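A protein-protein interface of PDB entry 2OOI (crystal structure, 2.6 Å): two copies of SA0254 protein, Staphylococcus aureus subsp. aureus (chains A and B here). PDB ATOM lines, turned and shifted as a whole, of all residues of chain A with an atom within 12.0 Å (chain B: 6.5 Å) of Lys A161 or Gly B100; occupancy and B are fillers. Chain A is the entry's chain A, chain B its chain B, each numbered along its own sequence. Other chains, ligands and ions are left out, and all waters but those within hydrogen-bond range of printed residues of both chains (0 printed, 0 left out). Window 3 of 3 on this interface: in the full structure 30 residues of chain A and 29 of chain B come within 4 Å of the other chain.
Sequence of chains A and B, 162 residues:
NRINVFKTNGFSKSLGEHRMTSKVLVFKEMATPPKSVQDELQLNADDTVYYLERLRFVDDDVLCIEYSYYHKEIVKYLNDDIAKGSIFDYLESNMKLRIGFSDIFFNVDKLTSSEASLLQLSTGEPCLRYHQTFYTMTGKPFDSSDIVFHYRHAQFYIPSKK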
ATOM      1  N   ASN A   4      23.149 -17.290  39.917  1.00  0.00           N
ATOM      2  CA  ASN A   4      24.320 -17.213  39.044  1.00  0.00           C
ATOM      3  C   ASN A   4      25.360 -18.299  39.349  1.00  0.00           C
ATOM      4  O   ASN A   4      25.854 -18.370  40.456  1.00  0.00           O
ATOM      5  CB  ASN A   4      24.955 -15.822  39.155  1.00  0.00           C
ATOM      6  CG  ASN A   4      26.020 -15.574  38.089  1.00  0.00           C
ATOM      7  OD1 ASN A   4      26.001 -16.195  37.028  1.00  0.00           O
ATOM      8  ND2 ASN A   4      26.951 -14.661  38.365  1.00  0.00           N
ATOM      9  N   PHE A   6      28.448 -19.022  37.633  1.00  0.00           N
ATOM     10  CA  PHE A   6      29.837 -18.823  37.236  1.00  0.00           C
ATOM     11  C   PHE A   6      30.762 -18.821  38.449  1.00  0.00           C
ATOM     12  O   PHE A   6      31.550 -19.747  38.641  1.00  0.00           O
ATOM     13  CB  PHE A   6      29.990 -17.515  36.457  1.00  0.00           C
ATOM     14  CG  PHE A   6      30.828 -17.643  35.217  1.00  0.00           C
ATOM     15  CD1 PHE A   6      30.891 -18.842  34.528  1.00  0.00           C
ATOM     16  CD2 PHE A   6      31.553 -16.563  34.741  1.00  0.00           C
ATOM     17  CE1 PHE A   6      31.661 -18.963  33.387  1.00  0.00           C
ATOM     18  CE2 PHE A   6      32.325 -16.679  33.600  1.00  0.00           C
ATOM     19  CZ  PHE A   6      32.379 -17.879  32.922  1.00  0.00           C
ATOM     20  N   LYS A   7      30.660 -17.776  39.263  1.00  0.00           N
ATOM     21  CA  LYS A   7      30.542 -17.939  40.708  1.00  0.00           C
ATOM     22  C   LYS A   7      31.003 -19.325  41.146  1.00  0.00           C
ATOM     23  O   LYS A   7      30.260 -20.301  41.036  1.00  0.00           O
ATOM     24  CB  LYS A   7      29.100 -17.698  41.157  1.00  0.00           C
ATOM     25  CG  LYS A   7      28.943 -16.564  42.156  1.00  0.00           C
ATOM     26  CD  LYS A   7      28.938 -15.212  41.461  1.00  0.00           C
ATOM     27  CE  LYS A   7      28.061 -14.214  42.199  1.00  0.00           C
ATOM     28  NZ  LYS A   7      27.761 -13.016  41.367  1.00  0.00           N
ATOM     29  N   TYR A 157      21.414 -18.288  35.550  1.00  0.00           N
ATOM     30  CA  TYR A 157      21.970 -17.302  34.660  1.00  0.00           C
ATOM     31  C   TYR A 157      23.465 -17.427  34.610  1.00  0.00           C
ATOM     32  O   TYR A 157      24.096 -17.730  35.603  1.00  0.00           O
ATOM     33  CB  TYR A 157      21.616 -15.890  35.127  1.00  0.00           C
ATOM     34  CG  TYR A 157      22.445 -14.840  34.423  1.00  0.00           C
ATOM     35  CD1 TYR A 157      22.248 -14.579  33.068  1.00  0.00           C
ATOM     36  CD2 TYR A 157      23.449 -14.133  35.094  1.00  0.00           C
ATOM     37  CE1 TYR A 157      23.016 -13.628  32.386  1.00  0.00           C
ATOM     38  CE2 TYR A 157      24.225 -13.183  34.436  1.00  0.00           C
ATOM     39  CZ  TYR A 157      24.002 -12.929  33.071  1.00  0.00           C
ATOM     40  OH  TYR A 157      24.748 -11.993  32.384  1.00  0.00           O
ATOM     41  N   ILE A 158      24.054 -17.179  33.452  1.00  0.00           N
ATOM     42  CA  ILE A 158      25.495 -17.003  33.418  1.00  0.00           C
ATOM     43  C   ILE A 158      25.889 -16.027  32.304  1.00  0.00           C
ATOM     44  O   ILE A 158      25.222 -15.967  31.287  1.00  0.00           O
ATOM     45  CB  ILE A 158      26.229 -18.365  33.429  1.00  0.00           C
ATOM     46  CG1 ILE A 158      25.990 -19.145  34.699  1.00  0.00           C
ATOM     47  CG2 ILE A 158      27.734 -18.222  33.229  1.00  0.00           C
ATOM     48  CD1 ILE A 158      26.524 -20.548  34.548  1.00  0.00           C
ATOM     49  N   PRO A 159      26.875 -15.150  32.563  1.00  0.00           N
ATOM     50  CA  PRO A 159      27.508 -14.309  31.532  1.00  0.00           C
ATOM     51  C   PRO A 159      28.828 -14.881  30.980  1.00  0.00           C
ATOM     52  O   PRO A 159      29.767 -15.128  31.760  1.00  0.00           O
ATOM     53  CB  PRO A 159      27.787 -12.999  32.279  1.00  0.00           C
ATOM     54  CG  PRO A 159      27.719 -13.336  33.762  1.00  0.00           C
ATOM     55  CD  PRO A 159      27.377 -14.801  33.905  1.00  0.00           C
ATOM     56  N   SER A 160      28.898 -15.046  29.653  1.00  0.00           N
ATOM     57  CA  SER A 160      30.058 -15.657  28.967  1.00  0.00           C
ATOM     58  C   SER A 160      30.969 -14.640  28.280  1.00  0.00           C
ATOM     59  O   SER A 160      30.608 -13.461  28.137  1.00  0.00           O
ATOM     60  CB  SER A 160      29.602 -16.653  27.902  1.00  0.00           C
ATOM     61  OG  SER A 160      28.902 -17.737  28.461  1.00  0.00           O
ATOM     62  N   LYS A 161      32.136 -15.135  27.836  1.00  0.00           N
ATOM     63  CA  LYS A 161      33.204 -14.308  27.277  1.00  0.00           C
ATOM     64  C   LYS A 161      34.121 -15.155  26.398  1.00  0.00           C
ATOM     65  O   LYS A 161      34.374 -14.809  25.242  1.00  0.00           O
ATOM     66  CB  LYS A 161      34.006 -13.646  28.418  1.00  0.00           C
ATOM     67  CG  LYS A 161      33.204 -12.595  29.230  1.00  0.00           C
ATOM     68  CD  LYS A 161      33.992 -11.893  30.385  1.00  0.00           C
ATOM     69  CE  LYS A 161      33.161 -10.854  31.194  1.00  0.00           C
ATOM     70  NZ  LYS A 161      33.885 -10.158  32.332  1.00  0.00           N
ATOM     71  N   PHE B   6      30.820 -22.700  29.242  1.00  0.00           N
ATOM     72  CA  PHE B   6      31.481 -21.626  29.975  1.00  0.00           C
ATOM     73  C   PHE B   6      31.566 -20.357  29.133  1.00  0.00           C
ATOM     74  O   PHE B   6      31.941 -19.296  29.631  1.00  0.00           O
ATOM     75  CB  PHE B   6      32.867 -22.064  30.421  1.00  0.00           C
ATOM     76  N   LYS B   7      31.216 -20.474  27.856  1.00  0.00           N
ATOM     77  CA  LYS B   7      32.183 -20.838  26.828  1.00  0.00           C
ATOM     78  C   LYS B   7      31.687 -20.444  25.441  1.00  0.00           C
ATOM     79  O   LYS B   7      31.242 -21.291  24.666  1.00  0.00           O
ATOM     80  CB  LYS B   7      32.477 -22.338  26.875  1.00  0.00           C
ATOM     81  CG  LYS B   7      33.359 -22.834  25.740  1.00  0.00           C
ATOM     82  CD  LYS B   7      33.983 -24.179  26.072  1.00  0.00           C
ATOM     83  CE  LYS B   7      34.762 -24.734  24.891  1.00  0.00           C
ATOM     84  NZ  LYS B   7      35.460 -26.004  25.232  1.00  0.00           N
ATOM     85  N   THR B   8      31.763 -19.153  25.134  1.00  0.00           N
ATOM     86  CA  THR B   8      30.808 -18.522  24.233  1.00  0.00           C
ATOM     87  C   THR B   8      31.143 -18.820  22.775  1.00  0.00           C
ATOM     88  O   THR B   8      31.663 -17.966  22.059  1.00  0.00           O
ATOM     89  CB  THR B   8      30.763 -16.996  24.436  1.00  0.00           C
ATOM     90  OG1 THR B   8      30.150 -16.377  23.299  1.00  0.00           O
ATOM     91  CG2 THR B   8      32.169 -16.440  24.614  1.00  0.00           C
ATOM     92  N   ARG B  98      32.912 -10.465  14.449  1.00  0.00           N
ATOM     93  CA  ARG B  98      33.620 -10.456  15.726  1.00  0.00           C
ATOM     94  C   ARG B  98      32.647 -10.731  16.861  1.00  0.00           C
ATOM     95  O   ARG B  98      31.865  -9.867  17.229  1.00  0.00           O
ATOM     96  CB  ARG B  98      34.334  -9.104  15.955  1.00  0.00           C
ATOM     97  CG  ARG B  98      35.414  -8.723  14.929  1.00  0.00           C
ATOM     98  CD  ARG B  98      36.150  -9.951  14.393  1.00  0.00           C
ATOM     99  NE  ARG B  98      37.280  -9.594  13.525  1.00  0.00           N
ATOM    100  CZ  ARG B  98      37.881 -10.413  12.653  1.00  0.00           C
ATOM    101  NH1 ARG B  98      37.472 -11.678  12.489  1.00  0.00           N
ATOM    102  NH2 ARG B  98      38.911  -9.961  11.940  1.00  0.00           N
ATOM    103  N   ILE B  99      32.701 -11.925  17.432  1.00  0.00           N
ATOM    104  CA  ILE B  99      31.754 -12.290  18.489  1.00  0.00           C
ATOM    105  C   ILE B  99      32.324 -11.979  19.869  1.00  0.00           C
ATOM    106  O   ILE B  99      33.366 -12.514  20.255  1.00  0.00           O
ATOM    107  CB  ILE B  99      31.325 -13.755  18.362  1.00  0.00           C
ATOM    108  CG1 ILE B  99      30.547 -13.916  17.038  1.00  0.00           C
ATOM    109  CG2 ILE B  99      30.479 -14.166  19.566  1.00  0.00           C
ATOM    110  CD1 ILE B  99      30.517 -15.310  16.453  1.00  0.00           C
ATOM    111  N   GLY B 100      31.629 -11.104  20.600  1.00  0.00           N
ATOM    112  CA  GLY B 100      32.119 -10.552  21.871  1.00  0.00           C
ATOM    113  C   GLY B 100      31.813 -11.364  23.126  1.00  0.00           C
ATOM    114  O   GLY B 100      32.734 -11.790  23.833  1.00  0.00           O
ATOM    115  N   PHE B 101      30.523 -11.562  23.410  1.00  0.00           N
ATOM    116  CA  PHE B 101      30.072 -12.209  24.647  1.00  0.00           C
ATOM    117  C   PHE B 101      28.623 -12.671  24.540  1.00  0.00           C
ATOM    118  O   PHE B 101      27.958 -12.396  23.554  1.00  0.00           O
ATOM    119  CB  PHE B 101      30.210 -11.244  25.830  1.00  0.00           C
ATOM    120  CG  PHE B 101      29.433  -9.954  25.679  1.00  0.00           C
ATOM    121  CD1 PHE B 101      28.163  -9.817  26.238  1.00  0.00           C
ATOM    122  CD2 PHE B 101      29.985  -8.863  25.003  1.00  0.00           C
ATOM    123  CE1 PHE B 101      27.448  -8.602  26.112  1.00  0.00           C
ATOM    124  CE2 PHE B 101      29.276  -7.660  24.874  1.00  0.00           C
ATOM    125  CZ  PHE B 101      28.010  -7.534  25.433  1.00  0.00           C
ATOM    126  N   SER B 102      28.131 -13.358  25.569  1.00  0.00           N
ATOM    127  CA  SER B 102      26.738 -13.776  25.587  1.00  0.00           C
ATOM    128  C   SER B 102      26.145 -13.887  26.986  1.00  0.00           C
ATOM    129  O   SER B 102      26.880 -14.007  27.976  1.00  0.00           O
ATOM    130  CB  SER B 102      26.587 -15.105  24.852  1.00  0.00           C
ATOM    131  OG  SER B 102      27.318 -16.122  25.490  1.00  0.00           O
ATOM    132  N   TYR B 135      26.272 -11.280  21.472  1.00  0.00           N
ATOM    133  CA  TYR B 135      26.567  -9.932  21.056  1.00  0.00           C
ATOM    134  C   TYR B 135      27.873  -9.916  20.311  1.00  0.00           C
ATOM    135  O   TYR B 135      28.784 -10.687  20.607  1.00  0.00           O
ATOM    136  CB  TYR B 135      26.686  -8.996  22.250  1.00  0.00           C
ATOM    137  CG  TYR B 135      25.477  -8.958  23.145  1.00  0.00           C
ATOM    138  CD1 TYR B 135      24.663  -7.827  23.216  1.00  0.00           C
ATOM    139  CD2 TYR B 135      25.153 -10.044  23.936  1.00  0.00           C
ATOM    140  CE1 TYR B 135      23.562  -7.797  24.047  1.00  0.00           C
ATOM    141  CE2 TYR B 135      24.062 -10.018  24.761  1.00  0.00           C
ATOM    142  CZ  TYR B 135      23.275  -8.895  24.812  1.00  0.00           C
ATOM    143  OH  TYR B 135      22.196  -8.912  25.647  1.00  0.00           O
ATOM    144  N   THR B 136      27.966  -9.003  19.359  1.00  0.00           N
ATOM    145  CA  THR B 136      29.220  -8.744  18.691  1.00  0.00           C
ATOM    146  C   THR B 136      30.168  -8.079  19.669  1.00  0.00           C
ATOM    147  O   THR B 136      29.769  -7.651  20.756  1.00  0.00           O
ATOM    148  CB  THR B 136      29.050  -7.776  17.539  1.00  0.00           C
ATOM    149  OG1 THR B 136      28.730  -6.486  18.071  1.00  0.00           O
ATOM    150  CG2 THR B 136      27.971  -8.259  16.587  1.00  0.00           C
ATOM    151  N   MET B 137      31.422  -7.953  19.257  1.00  0.00           N
ATOM    152  CA  MET B 137      32.450  -7.362  20.107  1.00  0.00           C
ATOM    153  C   MET B 137      32.218  -5.865  20.337  1.00  0.00           C
ATOM    154  O   MET B 137      32.886  -5.277  21.167  1.00  0.00           O
ATOM    155  CB  MET B 137      33.838  -7.596  19.514  1.00  0.00           C
ATOM    156  CG  MET B 137      34.910  -7.957  20.556  1.00  0.00           C
ATOM    157  SD  MET B 137      36.352  -8.703  19.744  1.00  0.00           S
ATOM    158  CE  MET B 137      35.657 -10.306  19.244  1.00  0.00           C
ATOM    159  N   THR B 138      31.284  -5.249  19.611  1.00  0.00           N
ATOM    160  CA  THR B 138      30.897  -3.867  19.902  1.00  0.00           C
ATOM    161  C   THR B 138      29.579  -3.785  20.693  1.00  0.00           C
ATOM    162  O   THR B 138      28.943  -2.735  20.742  1.00  0.00           O
ATOM    163  CB  THR B 138      30.803  -3.018  18.596  1.00  0.00           C
ATOM    164  OG1 THR B 138      30.122  -3.763  17.582  1.00  0.00           O
ATOM    165  CG2 THR B 138      32.189  -2.653  18.093  1.00  0.00           C
ATOM    166  N   GLY B 139      29.166  -4.889  21.310  1.00  0.00           N
ATOM    167  CA  GLY B 139      27.921  -4.918  22.083  1.00  0.00           C
ATOM    168  C   GLY B 139      26.612  -4.986  21.299  1.00  0.00           C
ATOM    169  O   GLY B 139      25.547  -4.709  21.849  1.00  0.00           O
ATOM    170  N   PHE B 142      23.060 -10.063  18.227  1.00  0.00           N
ATOM    171  CA  PHE B 142      22.710 -10.500  16.873  1.00  0.00           C
ATOM    172  C   PHE B 142      21.975 -11.838  16.765  1.00  0.00           C
ATOM    173  O   PHE B 142      21.446 -12.152  15.696  1.00  0.00           O
ATOM    174  CB  PHE B 142      23.961 -10.524  16.004  1.00  0.00           C
ATOM    175  CG  PHE B 142      24.948 -11.558  16.406  1.00  0.00           C
ATOM    176  CD1 PHE B 142      24.829 -12.848  15.957  1.00  0.00           C
ATOM    177  CD2 PHE B 142      25.985 -11.247  17.262  1.00  0.00           C
ATOM    178  CE1 PHE B 142      25.729 -13.818  16.343  1.00  0.00           C
ATOM    179  CE2 PHE B 142      26.902 -12.231  17.668  1.00  0.00           C
ATOM    180  CZ  PHE B 142      26.765 -13.512  17.203  1.00  0.00           C
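Hydrophobic or aromatic side chains of chain A that line the printed part of chain B: Phe A6. Printed residues of chain B that touch a printed residue of chain A: Phe B6, Lys B7, Thr B8, Gly B100, Phe B101 and Ser B102. Among the printed residues, 9 pairs touch across the chains.
Phe B6 touches its own counterpart, Phe A6.
N of Ser A160 lies within hydrogen-bond range of O of Ser B102.
Printed residues of chain B within 4 Å of Phe A6: Phe B6. Of the printed residues of chain B, Lys A161 touches Thr B8 and Gly B100. Of chain A, only Phe A6 (3.6 Å) and Ser A160 (3.6 Å) come within 4 Å of Phe B6. Printed residues of chain A within 4 Å of Lys B7: Ser A160. Of chain A, only Ser A160 (3.7 Å) and Lys A161 (2.8 Å) come within 4 Å of Thr B8. No residue of chain A comes within 4 Å of Ile B99. Printed residues of chain A within 4 Å of Gly B100: Lys A161. The nearest printed residue of chain B that does not touch Lys A161 is Phe B101 (4.5 Å).
Among the printed residues, pairs that only touch across the chains: Lys A161 with Thr B8 (2.8 Å), Ser A160 with Phe B101 (3.2 Å), Phe A6 with Phe B6 (3.6 Å), Ser A160 with Phe B6 (3.6 Å), Pro A159 with Ser B102 (3.6 Å), Ser A160 with Lys B7 (3.6 Å), Ser A160 with Thr B8 (3.7 Å) and Lys A161 with Gly B100 (3.7 Å).
The backbone NH (N) of Gly B100 is in hydrogen-bond range of the backbone carbonyl oxygen (O) of Tyr B135, 2.9 Å away. The backbone carbonyl oxygen (O) of Phe B101 sits at hydrogen-bond distance from the backbone NH (N) of Tyr B135.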
